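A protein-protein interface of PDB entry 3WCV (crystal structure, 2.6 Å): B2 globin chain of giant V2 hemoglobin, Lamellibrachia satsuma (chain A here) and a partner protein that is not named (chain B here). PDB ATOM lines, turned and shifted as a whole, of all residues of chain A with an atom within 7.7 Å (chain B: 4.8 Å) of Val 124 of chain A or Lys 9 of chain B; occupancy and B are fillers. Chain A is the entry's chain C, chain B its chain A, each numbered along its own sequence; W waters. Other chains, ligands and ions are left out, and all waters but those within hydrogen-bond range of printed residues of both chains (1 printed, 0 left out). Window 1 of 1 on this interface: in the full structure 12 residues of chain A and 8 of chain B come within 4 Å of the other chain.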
ATOM      1  N   MET A  16       8.866 -19.281 -13.771  1.00  0.00           N
ATOM      2  CA  MET A  16      10.184 -19.882 -13.804  1.00  0.00           C
ATOM      3  C   MET A  16      11.244 -18.833 -14.018  1.00  0.00           C
ATOM      4  O   MET A  16      12.369 -18.987 -13.553  1.00  0.00           O
ATOM      5  CB  MET A  16      10.255 -20.892 -14.943  1.00  0.00           C
ATOM      6  CG  MET A  16       9.255 -22.041 -14.839  1.00  0.00           C
ATOM      7  SD  MET A  16       9.482 -23.208 -16.228  1.00  0.00           S
ATOM      8  CE  MET A  16       8.062 -22.850 -17.232  1.00  0.00           C
ATOM      9  N   ASN A  19      11.516 -15.839 -11.018  1.00  0.00           N
ATOM     10  CA  ASN A  19      12.211 -16.409  -9.895  1.00  0.00           C
ATOM     11  C   ASN A  19      13.710 -16.239 -10.044  1.00  0.00           C
ATOM     12  O   ASN A  19      14.359 -15.575  -9.228  1.00  0.00           O
ATOM     13  CB  ASN A  19      11.850 -17.898  -9.787  1.00  0.00           C
ATOM     14  CG  ASN A  19      12.984 -18.752  -9.226  1.00  0.00           C
ATOM     15  OD1 ASN A  19      12.966 -19.152  -8.066  1.00  0.00           O
ATOM     16  ND2 ASN A  19      13.976 -19.031 -10.062  1.00  0.00           N
ATOM     17  N   VAL A  20      14.261 -16.832 -11.095  1.00  0.00           N
ATOM     18  CA  VAL A  20      15.687 -16.771 -11.327  1.00  0.00           C
ATOM     19  C   VAL A  20      16.133 -15.439 -11.932  1.00  0.00           C
ATOM     20  O   VAL A  20      17.242 -15.307 -12.440  1.00  0.00           O
ATOM     21  CB  VAL A  20      16.097 -17.981 -12.200  1.00  0.00           C
ATOM     22  CG1 VAL A  20      16.577 -17.541 -13.556  1.00  0.00           C
ATOM     23  CG2 VAL A  20      17.139 -18.782 -11.470  1.00  0.00           C
ATOM     24  N   TRP A  21      15.269 -14.436 -11.835  1.00  0.00           N
ATOM     25  CA  TRP A  21      15.578 -13.115 -12.360  1.00  0.00           C
ATOM     26  C   TRP A  21      15.872 -12.094 -11.265  1.00  0.00           C
ATOM     27  O   TRP A  21      15.038 -11.826 -10.391  1.00  0.00           O
ATOM     28  CB  TRP A  21      14.419 -12.623 -13.224  1.00  0.00           C
ATOM     29  CG  TRP A  21      14.541 -11.203 -13.645  1.00  0.00           C
ATOM     30  CD1 TRP A  21      14.059 -10.103 -12.993  1.00  0.00           C
ATOM     31  CD2 TRP A  21      15.173 -10.720 -14.832  1.00  0.00           C
ATOM     32  NE1 TRP A  21      14.341  -8.964 -13.710  1.00  0.00           N
ATOM     33  CE2 TRP A  21      15.027  -9.314 -14.844  1.00  0.00           C
ATOM     34  CE3 TRP A  21      15.848 -11.340 -15.892  1.00  0.00           C
ATOM     35  CZ2 TRP A  21      15.531  -8.515 -15.879  1.00  0.00           C
ATOM     36  CZ3 TRP A  21      16.351 -10.547 -16.921  1.00  0.00           C
ATOM     37  CH2 TRP A  21      16.191  -9.149 -16.906  1.00  0.00           C
ATOM     38  N   ARG A  28      23.014 -12.611 -11.422  1.00  0.00           N
ATOM     39  CA  ARG A  28      22.204 -13.754 -11.817  1.00  0.00           C
ATOM     40  C   ARG A  28      21.987 -13.834 -13.348  1.00  0.00           C
ATOM     41  O   ARG A  28      22.264 -14.858 -13.963  1.00  0.00           O
ATOM     42  CB  ARG A  28      20.861 -13.708 -11.063  1.00  0.00           C
ATOM     43  CG  ARG A  28      20.325 -15.065 -10.601  1.00  0.00           C
ATOM     44  CD  ARG A  28      19.884 -15.016  -9.137  1.00  0.00           C
ATOM     45  NE  ARG A  28      18.948 -13.922  -8.880  1.00  0.00           N
ATOM     46  CZ  ARG A  28      18.645 -13.448  -7.667  1.00  0.00           C
ATOM     47  NH1 ARG A  28      17.780 -12.448  -7.536  1.00  0.00           N
ATOM     48  NH2 ARG A  28      19.206 -13.970  -6.586  1.00  0.00           N
ATOM     49  N   ALA A  31      25.173 -14.635 -15.286  1.00  0.00           N
ATOM     50  CA  ALA A  31      25.556 -16.011 -15.071  1.00  0.00           C
ATOM     51  C   ALA A  31      24.739 -16.946 -15.945  1.00  0.00           C
ATOM     52  O   ALA A  31      25.253 -17.907 -16.501  1.00  0.00           O
ATOM     53  CB  ALA A  31      25.367 -16.355 -13.624  1.00  0.00           C
ATOM     54  N   ILE A  32      23.445 -16.677 -16.044  1.00  0.00           N
ATOM     55  CA  ILE A  32      22.563 -17.528 -16.835  1.00  0.00           C
ATOM     56  C   ILE A  32      22.909 -17.468 -18.322  1.00  0.00           C
ATOM     57  O   ILE A  32      22.987 -18.491 -19.008  1.00  0.00           O
ATOM     58  CB  ILE A  32      21.101 -17.106 -16.633  1.00  0.00           C
ATOM     59  CG1 ILE A  32      20.709 -17.352 -15.180  1.00  0.00           C
ATOM     60  CG2 ILE A  32      20.199 -17.842 -17.610  1.00  0.00           C
ATOM     61  CD1 ILE A  32      19.366 -16.807 -14.829  1.00  0.00           C
ATOM     62  N   ALA A  35      26.441 -19.004 -19.269  1.00  0.00           N
ATOM     63  CA  ALA A  35      26.281 -20.451 -19.239  1.00  0.00           C
ATOM     64  C   ALA A  35      25.532 -20.957 -20.459  1.00  0.00           C
ATOM     65  O   ALA A  35      25.793 -22.063 -20.943  1.00  0.00           O
ATOM     66  CB  ALA A  35      25.550 -20.869 -17.976  1.00  0.00           C
ATOM     67  N   PHE A 117      19.247 -23.504 -23.356  1.00  0.00           N
ATOM     68  CA  PHE A 117      18.427 -22.986 -22.268  1.00  0.00           C
ATOM     69  C   PHE A 117      17.800 -24.122 -21.487  1.00  0.00           C
ATOM     70  O   PHE A 117      17.743 -24.075 -20.266  1.00  0.00           O
ATOM     71  CB  PHE A 117      17.345 -22.054 -22.808  1.00  0.00           C
ATOM     72  CG  PHE A 117      17.765 -20.621 -22.858  1.00  0.00           C
ATOM     73  CD1 PHE A 117      17.786 -19.853 -21.708  1.00  0.00           C
ATOM     74  CD2 PHE A 117      18.169 -20.042 -24.057  1.00  0.00           C
ATOM     75  CE1 PHE A 117      18.206 -18.518 -21.752  1.00  0.00           C
ATOM     76  CE2 PHE A 117      18.589 -18.709 -24.108  1.00  0.00           C
ATOM     77  CZ  PHE A 117      18.608 -17.947 -22.956  1.00  0.00           C
ATOM     78  N   ARG A 119      19.016 -26.860 -20.884  1.00  0.00           N
ATOM     79  CA  ARG A 119      20.037 -27.514 -20.056  1.00  0.00           C
ATOM     80  C   ARG A 119      20.503 -26.624 -18.898  1.00  0.00           C
ATOM     81  O   ARG A 119      20.860 -27.109 -17.823  1.00  0.00           O
ATOM     82  CB  ARG A 119      21.250 -27.918 -20.909  1.00  0.00           C
ATOM     83  CG  ARG A 119      21.147 -29.290 -21.553  1.00  0.00           C
ATOM     84  CD  ARG A 119      22.468 -29.685 -22.213  1.00  0.00           C
ATOM     85  NE  ARG A 119      22.811 -28.826 -23.349  1.00  0.00           N
ATOM     86  CZ  ARG A 119      22.399 -29.039 -24.597  1.00  0.00           C
ATOM     87  NH1 ARG A 119      22.752 -28.204 -25.571  1.00  0.00           N
ATOM     88  NH2 ARG A 119      21.643 -30.095 -24.875  1.00  0.00           N
ATOM     89  N   VAL A 120      20.498 -25.322 -19.134  1.00  0.00           N
ATOM     90  CA  VAL A 120      20.903 -24.333 -18.142  1.00  0.00           C
ATOM     91  C   VAL A 120      19.810 -24.052 -17.076  1.00  0.00           C
ATOM     92  O   VAL A 120      20.072 -24.136 -15.869  1.00  0.00           O
ATOM     93  CB  VAL A 120      21.281 -23.019 -18.865  1.00  0.00           C
ATOM     94  CG1 VAL A 120      21.603 -21.923 -17.886  1.00  0.00           C
ATOM     95  CG2 VAL A 120      22.461 -23.271 -19.749  1.00  0.00           C
ATOM     96  N   MET A 121      18.600 -23.726 -17.526  1.00  0.00           N
ATOM     97  CA  MET A 121      17.502 -23.404 -16.626  1.00  0.00           C
ATOM     98  C   MET A 121      17.303 -24.352 -15.434  1.00  0.00           C
ATOM     99  O   MET A 121      17.395 -23.933 -14.279  1.00  0.00           O
ATOM    100  CB  MET A 121      16.197 -23.299 -17.413  1.00  0.00           C
ATOM    101  CG  MET A 121      16.080 -22.079 -18.296  1.00  0.00           C
ATOM    102  SD  MET A 121      16.390 -20.510 -17.489  1.00  0.00           S
ATOM    103  CE  MET A 121      14.957 -20.348 -16.521  1.00  0.00           C
ATOM    104  N   PRO A 122      17.035 -25.638 -15.702  1.00  0.00           N
ATOM    105  CA  PRO A 122      16.839 -26.554 -14.578  1.00  0.00           C
ATOM    106  C   PRO A 122      17.918 -26.505 -13.492  1.00  0.00           C
ATOM    107  O   PRO A 122      17.649 -26.836 -12.343  1.00  0.00           O
ATOM    108  CB  PRO A 122      16.741 -27.926 -15.258  1.00  0.00           C
ATOM    109  CG  PRO A 122      17.568 -27.753 -16.490  1.00  0.00           C
ATOM    110  CD  PRO A 122      17.173 -26.379 -16.967  1.00  0.00           C
ATOM    111  N   GLN A 123      19.126 -26.080 -13.842  1.00  0.00           N
ATOM    112  CA  GLN A 123      20.221 -26.021 -12.872  1.00  0.00           C
ATOM    113  C   GLN A 123      20.106 -24.812 -11.958  1.00  0.00           C
ATOM    114  O   GLN A 123      20.518 -24.850 -10.797  1.00  0.00           O
ATOM    115  CB  GLN A 123      21.561 -25.942 -13.590  1.00  0.00           C
ATOM    116  CG  GLN A 123      21.961 -27.173 -14.345  1.00  0.00           C
ATOM    117  CD  GLN A 123      23.256 -26.953 -15.056  1.00  0.00           C
ATOM    118  OE1 GLN A 123      24.263 -26.614 -14.437  1.00  0.00           O
ATOM    119  NE2 GLN A 123      23.242 -27.122 -16.373  1.00  0.00           N
ATOM    120  N   VAL A 124      19.538 -23.747 -12.488  1.00  0.00           N
ATOM    121  CA  VAL A 124      19.405 -22.517 -11.739  1.00  0.00           C
ATOM    122  C   VAL A 124      17.973 -22.231 -11.251  1.00  0.00           C
ATOM    123  O   VAL A 124      17.787 -21.623 -10.204  1.00  0.00           O
ATOM    124  CB  VAL A 124      19.966 -21.352 -12.607  1.00  0.00           C
ATOM    125  CG1 VAL A 124      19.117 -21.187 -13.861  1.00  0.00           C
ATOM    126  CG2 VAL A 124      20.059 -20.084 -11.806  1.00  0.00           C
ATOM    127  N   ALA A 125      16.969 -22.683 -11.997  1.00  0.00           N
ATOM    128  CA  ALA A 125      15.568 -22.465 -11.635  1.00  0.00           C
ATOM    129  C   ALA A 125      14.922 -23.613 -10.849  1.00  0.00           C
ATOM    130  O   ALA A 125      15.106 -24.792 -11.160  1.00  0.00           O
ATOM    131  CB  ALA A 125      14.750 -22.195 -12.873  1.00  0.00           C
ATOM    132  N   SER A 126      14.151 -23.243  -9.834  1.00  0.00           N
ATOM    133  CA  SER A 126      13.457 -24.209  -8.996  1.00  0.00           C
ATOM    134  C   SER A 126      12.069 -24.497  -9.583  1.00  0.00           C
ATOM    135  O   SER A 126      11.380 -23.584 -10.035  1.00  0.00           O
ATOM    136  CB  SER A 126      13.298 -23.661  -7.565  1.00  0.00           C
ATOM    137  OG  SER A 126      14.539 -23.357  -6.954  1.00  0.00           O
ATOM    138  N   CYS A 127      11.653 -25.756  -9.578  1.00  0.00           N
ATOM    139  CA  CYS A 127      10.332 -26.103 -10.108  1.00  0.00           C
ATOM    140  C   CYS A 127      10.271 -25.783 -11.609  1.00  0.00           C
ATOM    141  O   CYS A 127       9.291 -25.216 -12.094  1.00  0.00           O
ATOM    142  CB  CYS A 127       9.216 -25.294  -9.419  1.00  0.00           C
ATOM    143  SG  CYS A 127       8.799 -25.539  -7.646  1.00  0.00           S
ATOM    144  N   PHE A 128      11.323 -26.133 -12.332  1.00  0.00           N
ATOM    145  CA  PHE A 128      11.362 -25.868 -13.762  1.00  0.00           C
ATOM    146  C   PHE A 128      10.462 -26.848 -14.511  1.00  0.00           C
ATOM    147  O   PHE A 128      10.510 -28.065 -14.275  1.00  0.00           O
ATOM    148  CB  PHE A 128      12.793 -25.979 -14.286  1.00  0.00           C
ATOM    149  CG  PHE A 128      12.928 -25.705 -15.758  1.00  0.00           C
ATOM    150  CD1 PHE A 128      12.717 -24.424 -16.264  1.00  0.00           C
ATOM    151  CD2 PHE A 128      13.295 -26.719 -16.638  1.00  0.00           C
ATOM    152  CE1 PHE A 128      12.869 -24.147 -17.624  1.00  0.00           C
ATOM    153  CE2 PHE A 128      13.449 -26.452 -17.994  1.00  0.00           C
ATOM    154  CZ  PHE A 128      13.233 -25.159 -18.486  1.00  0.00           C
ATOM    155  N   LEU B   5      25.931 -21.971 -11.280  1.00  0.00           N
ATOM    156  CA  LEU B   5      24.481 -22.125 -11.403  1.00  0.00           C
ATOM    157  C   LEU B   5      23.912 -22.751 -10.125  1.00  0.00           C
ATOM    158  O   LEU B   5      22.903 -22.285  -9.611  1.00  0.00           O
ATOM    159  CB  LEU B   5      24.124 -22.988 -12.622  1.00  0.00           C
ATOM    160  CG  LEU B   5      24.571 -22.500 -14.011  1.00  0.00           C
ATOM    161  CD1 LEU B   5      23.890 -23.340 -15.071  1.00  0.00           C
ATOM    162  CD2 LEU B   5      24.222 -21.041 -14.219  1.00  0.00           C
ATOM    163  N   GLN B   6      24.557 -23.801  -9.620  1.00  0.00           N
ATOM    164  CA  GLN B   6      24.122 -24.441  -8.383  1.00  0.00           C
ATOM    165  C   GLN B   6      24.278 -23.495  -7.189  1.00  0.00           C
ATOM    166  O   GLN B   6      23.503 -23.567  -6.239  1.00  0.00           O
ATOM    167  CB  GLN B   6      24.914 -25.730  -8.138  1.00  0.00           C
ATOM    168  CG  GLN B   6      24.895 -26.649  -9.344  1.00  0.00           C
ATOM    169  CD  GLN B   6      25.368 -28.061  -9.047  1.00  0.00           C
ATOM    170  OE1 GLN B   6      26.509 -28.279  -8.599  1.00  0.00           O
ATOM    171  NE2 GLN B   6      24.498 -29.041  -9.306  1.00  0.00           N
ATOM    172  N   ARG B   7      25.266 -22.605  -7.234  1.00  0.00           N
ATOM    173  CA  ARG B   7      25.462 -21.661  -6.135  1.00  0.00           C
ATOM    174  C   ARG B   7      24.311 -20.664  -6.103  1.00  0.00           C
ATOM    175  O   ARG B   7      23.871 -20.260  -5.027  1.00  0.00           O
ATOM    176  CB  ARG B   7      26.803 -20.924  -6.269  1.00  0.00           C
ATOM    177  CG  ARG B   7      27.996 -21.856  -6.158  1.00  0.00           C
ATOM    178  CD  ARG B   7      29.343 -21.141  -6.256  1.00  0.00           C
ATOM    179  NE  ARG B   7      30.424 -22.119  -6.075  1.00  0.00           N
ATOM    180  CZ  ARG B   7      31.543 -21.905  -5.383  1.00  0.00           C
ATOM    181  NH1 ARG B   7      31.763 -20.733  -4.791  1.00  0.00           N
ATOM    182  NH2 ARG B   7      32.430 -22.882  -5.262  1.00  0.00           N
ATOM    183  N   LEU B   8      23.813 -20.286  -7.278  1.00  0.00           N
ATOM    184  CA  LEU B   8      22.697 -19.348  -7.360  1.00  0.00           C
ATOM    185  C   LEU B   8      21.398 -20.041  -6.921  1.00  0.00           C
ATOM    186  O   LEU B   8      20.555 -19.456  -6.241  1.00  0.00           O
ATOM    187  CB  LEU B   8      22.549 -18.838  -8.796  1.00  0.00           C
ATOM    188  CG  LEU B   8      23.698 -17.967  -9.315  1.00  0.00           C
ATOM    189  CD1 LEU B   8      23.501 -17.661 -10.805  1.00  0.00           C
ATOM    190  CD2 LEU B   8      23.769 -16.682  -8.488  1.00  0.00           C
ATOM    191  N   LYS B   9      21.261 -21.294  -7.326  1.00  0.00           N
ATOM    192  CA  LYS B   9      20.109 -22.108  -6.999  1.00  0.00           C
ATOM    193  C   LYS B   9      20.009 -22.195  -5.488  1.00  0.00           C
ATOM    194  O   LYS B   9      18.969 -21.918  -4.900  1.00  0.00           O
ATOM    195  CB  LYS B   9      20.324 -23.497  -7.565  1.00  0.00           C
ATOM    196  CG  LYS B   9      19.130 -24.391  -7.455  1.00  0.00           C
ATOM    197  CD  LYS B   9      17.958 -23.821  -8.233  1.00  0.00           C
ATOM    198  CE  LYS B   9      17.078 -24.924  -8.682  1.00  0.00           C
ATOM    199  NZ  LYS B   9      17.869 -25.911  -9.437  1.00  0.00           N
ATOM    200  N   VAL B  10      21.129 -22.595  -4.879  1.00  0.00           N
ATOM    201  CA  VAL B  10      21.245 -22.754  -3.439  1.00  0.00           C
ATOM    202  C   VAL B  10      20.916 -21.445  -2.726  1.00  0.00           C
ATOM    203  O   VAL B  10      20.197 -21.461  -1.726  1.00  0.00           O
ATOM    204  CB  VAL B  10      22.682 -23.271  -3.057  1.00  0.00           C
ATOM    205  CG1 VAL B  10      22.947 -23.127  -1.569  1.00  0.00           C
ATOM    206  CG2 VAL B  10      22.809 -24.741  -3.450  1.00  0.00           C
ATOM    207  N   LYS B  11      21.437 -20.324  -3.233  1.00  0.00           N
ATOM    208  CA  LYS B  11      21.158 -19.018  -2.637  1.00  0.00           C
ATOM    209  C   LYS B  11      19.665 -18.728  -2.629  1.00  0.00           C
ATOM    210  O   LYS B  11      19.134 -18.262  -1.629  1.00  0.00           O
ATOM    211  CB  LYS B  11      21.898 -17.902  -3.378  1.00  0.00           C
ATOM    212  CG  LYS B  11      23.369 -17.850  -3.017  1.00  0.00           C
ATOM    213  CD  LYS B  11      24.098 -16.654  -3.641  1.00  0.00           C
ATOM    214  CE  LYS B  11      23.668 -15.347  -2.990  1.00  0.00           C
ATOM    215  NZ  LYS B  11      24.364 -14.185  -3.603  1.00  0.00           N
ATOM    216  N   MET B  12      18.996 -19.024  -3.739  1.00  0.00           N
ATOM    217  CA  MET B  12      17.565 -18.814  -3.862  1.00  0.00           C
ATOM    218  C   MET B  12      16.853 -19.669  -2.828  1.00  0.00           C
ATOM    219  O   MET B  12      16.169 -19.163  -1.937  1.00  0.00           O
ATOM    220  CB  MET B  12      17.083 -19.253  -5.231  1.00  0.00           C
ATOM    221  CG  MET B  12      17.822 -18.627  -6.377  1.00  0.00           C
ATOM    222  SD  MET B  12      17.382 -16.921  -6.629  1.00  0.00           S
ATOM    223  CE  MET B  12      17.351 -16.873  -8.437  1.00  0.00           C
ATOM    224  N   GLN B  13      17.017 -20.978  -2.952  1.00  0.00           N
ATOM    225  CA  GLN B  13      16.335 -21.871  -2.045  1.00  0.00           C
ATOM    226  C   GLN B  13      16.627 -21.567  -0.564  1.00  0.00           C
ATOM    227  O   GLN B  13      15.723 -21.618   0.276  1.00  0.00           O
ATOM    228  CB  GLN B  13      16.672 -23.325  -2.384  1.00  0.00           C
ATOM    229  CG  GLN B  13      16.491 -23.676  -3.839  1.00  0.00           C
ATOM    230  CD  GLN B  13      16.243 -25.161  -4.071  1.00  0.00           C
ATOM    231  OE1 GLN B  13      16.762 -26.021  -3.340  1.00  0.00           O
ATOM    232  NE2 GLN B  13      15.457 -25.475  -5.097  1.00  0.00           N
ATOM    233  N   ASP B 124      16.587 -28.754  -4.596  1.00  0.00           N
ATOM    234  CA  ASP B 124      17.591 -29.346  -5.468  1.00  0.00           C
ATOM    235  C   ASP B 124      18.622 -30.035  -4.594  1.00  0.00           C
ATOM    236  O   ASP B 124      19.681 -29.460  -4.311  1.00  0.00           O
ATOM    237  CB  ASP B 124      18.276 -28.242  -6.283  1.00  0.00           C
ATOM    238  CG  ASP B 124      19.043 -28.776  -7.481  1.00  0.00           C
ATOM    239  OD1 ASP B 124      19.654 -29.872  -7.384  1.00  0.00           O
ATOM    240  OD2 ASP B 124      19.042 -28.069  -8.518  1.00  0.00           O
ATOM    241  N   ALA B 127      22.378 -30.291  -5.900  1.00  0.00           N
ATOM    242  CA  ALA B 127      23.038 -28.997  -5.833  1.00  0.00           C
ATOM    243  C   ALA B 127      23.479 -28.682  -4.405  1.00  0.00           C
ATOM    244  O   ALA B 127      24.557 -28.096  -4.183  1.00  0.00           O
ATOM    245  CB  ALA B 127      22.111 -27.916  -6.334  1.00  0.00           C
HETATM  246  O   HOH W   1      21.385 -27.265  -9.796  1.00  0.00           O
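Trp 21 of chain A touches none of the printed residues of chain B.
Of the printed residues of chain B, Ala 35 of chain A touches Leu 5.
Phe 117 of chain A touches none of the printed residues of chain B.
Val 124 of chain A touches just one residue of chain B: Lys 9.
Of the printed residues of chain B, Ser 126 of chain A touches Lys 9 and Gln 13.
Of the printed residues of chain A, Leu 5 of chain B touches Ala 35, Val 120 and Gln 123.
Of chain A, only Pro 122, Gln 123, Val 124, Ala 125 and Ser 126 come within 4 Å of Lys 9 of chain B.
Printed residues of chain A within 4 Å of Gln 13 of chain B: Ser 126 (3.0 Å).
The nearest printed residue of chain B that does not touch Val 124 of chain A is Leu 8 of chain B (4.1 Å).
The nearest printed residue of chain A that does not touch Leu 5 of chain B is Ala 31 of chain A (4.01 Å).
NZ of Lys 9 of chain B lies within salt-bridge range of OD2 of Asp 124 of chain B (2.6 Å).
The backbone carbonyl oxygen (O) of Arg 119 of chain A sits at hydrogen-bond distance from the side-chain amide nitrogen (NE2) of Gln 123 of chain A (2.8 Å).
OE1 of Gln 13 of chain B sits at hydrogen-bond distance from N of Asp 124 of chain B, at 3.0 Å.
Water W1 bridges the backbone carbonyl oxygen of Gln 123 of chain A and the side-chain carboxylate of Asp 124 of chain B.
Printed residues of chain B that touch a printed residue of chain A: Leu 5, Leu 8, Lys 9, Met 12 and Gln 13.
Hydrophobic or aromatic side chains of chain B within 4 Å of the printed part of chain A: Leu 5, Leu 8 and Met 12.
Of the 19 printed residues of chain A, 11 touch a printed residue of chain B.
Hydrophobic or aromatic side chains of chain A that line the printed part of chain B: Val 20, Ala 31, Ala 35 and Val 120.
Among the printed residues, 13 pairs touch across the chains.
The side-chain sulfur (SD) of Met 12 of chain B sits at hydrogen-bond distance from the guanidinium group (NH2) of Arg 28 of chain A, at 3.5 Å.
The side-chain amino group (NZ) of Lys 9 of chain B lies within hydrogen-bond range of the backbone carbonyl oxygen (O) of Pro 122 of chain A (3.1 Å).
The side-chain amino group (NZ) of Lys 9 of chain B lies close to the backbone carbonyl oxygen (O) of Ala 125 of chain A.
The side-chain amino group (NZ) of Lys 9 of chain B sits at hydrogen-bond distance from the backbone carbonyl oxygen (O) of Gln 123 of chain A, at 3.2 Å.
The side-chain hydroxyl (OG) of Ser 126 of chain A sits at hydrogen-bond distance from the side-chain amide nitrogen (NE2) of Gln 13 of chain B, at 3.0 Å.
CE of Met 12 of chain B touches O of Asn 19 of chain A (3.4 Å).
CE of Met 12 of chain B touches CA of Val 20 of chain A, at 3.3 Å.
Leu 8 of chain B touches Ala 31 of chain A (CD1 to CB, 3.6 Å).
Ala 35 of chain A touches Leu 5 of chain B (CB to CD2, 3.99 Å).
Leu 5 of chain B touches Val 120 of chain A (CD1 to CG1, 3.9 Å).
Gln 123 of chain A touches Leu 5 of chain B.
O of Val 124 of chain A touches CD of Lys 9 of chain B, at 3.0 Å.
OG of Ser 126 of chain A touches CE of Lys 9 of chain B, at 3.4 Å.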
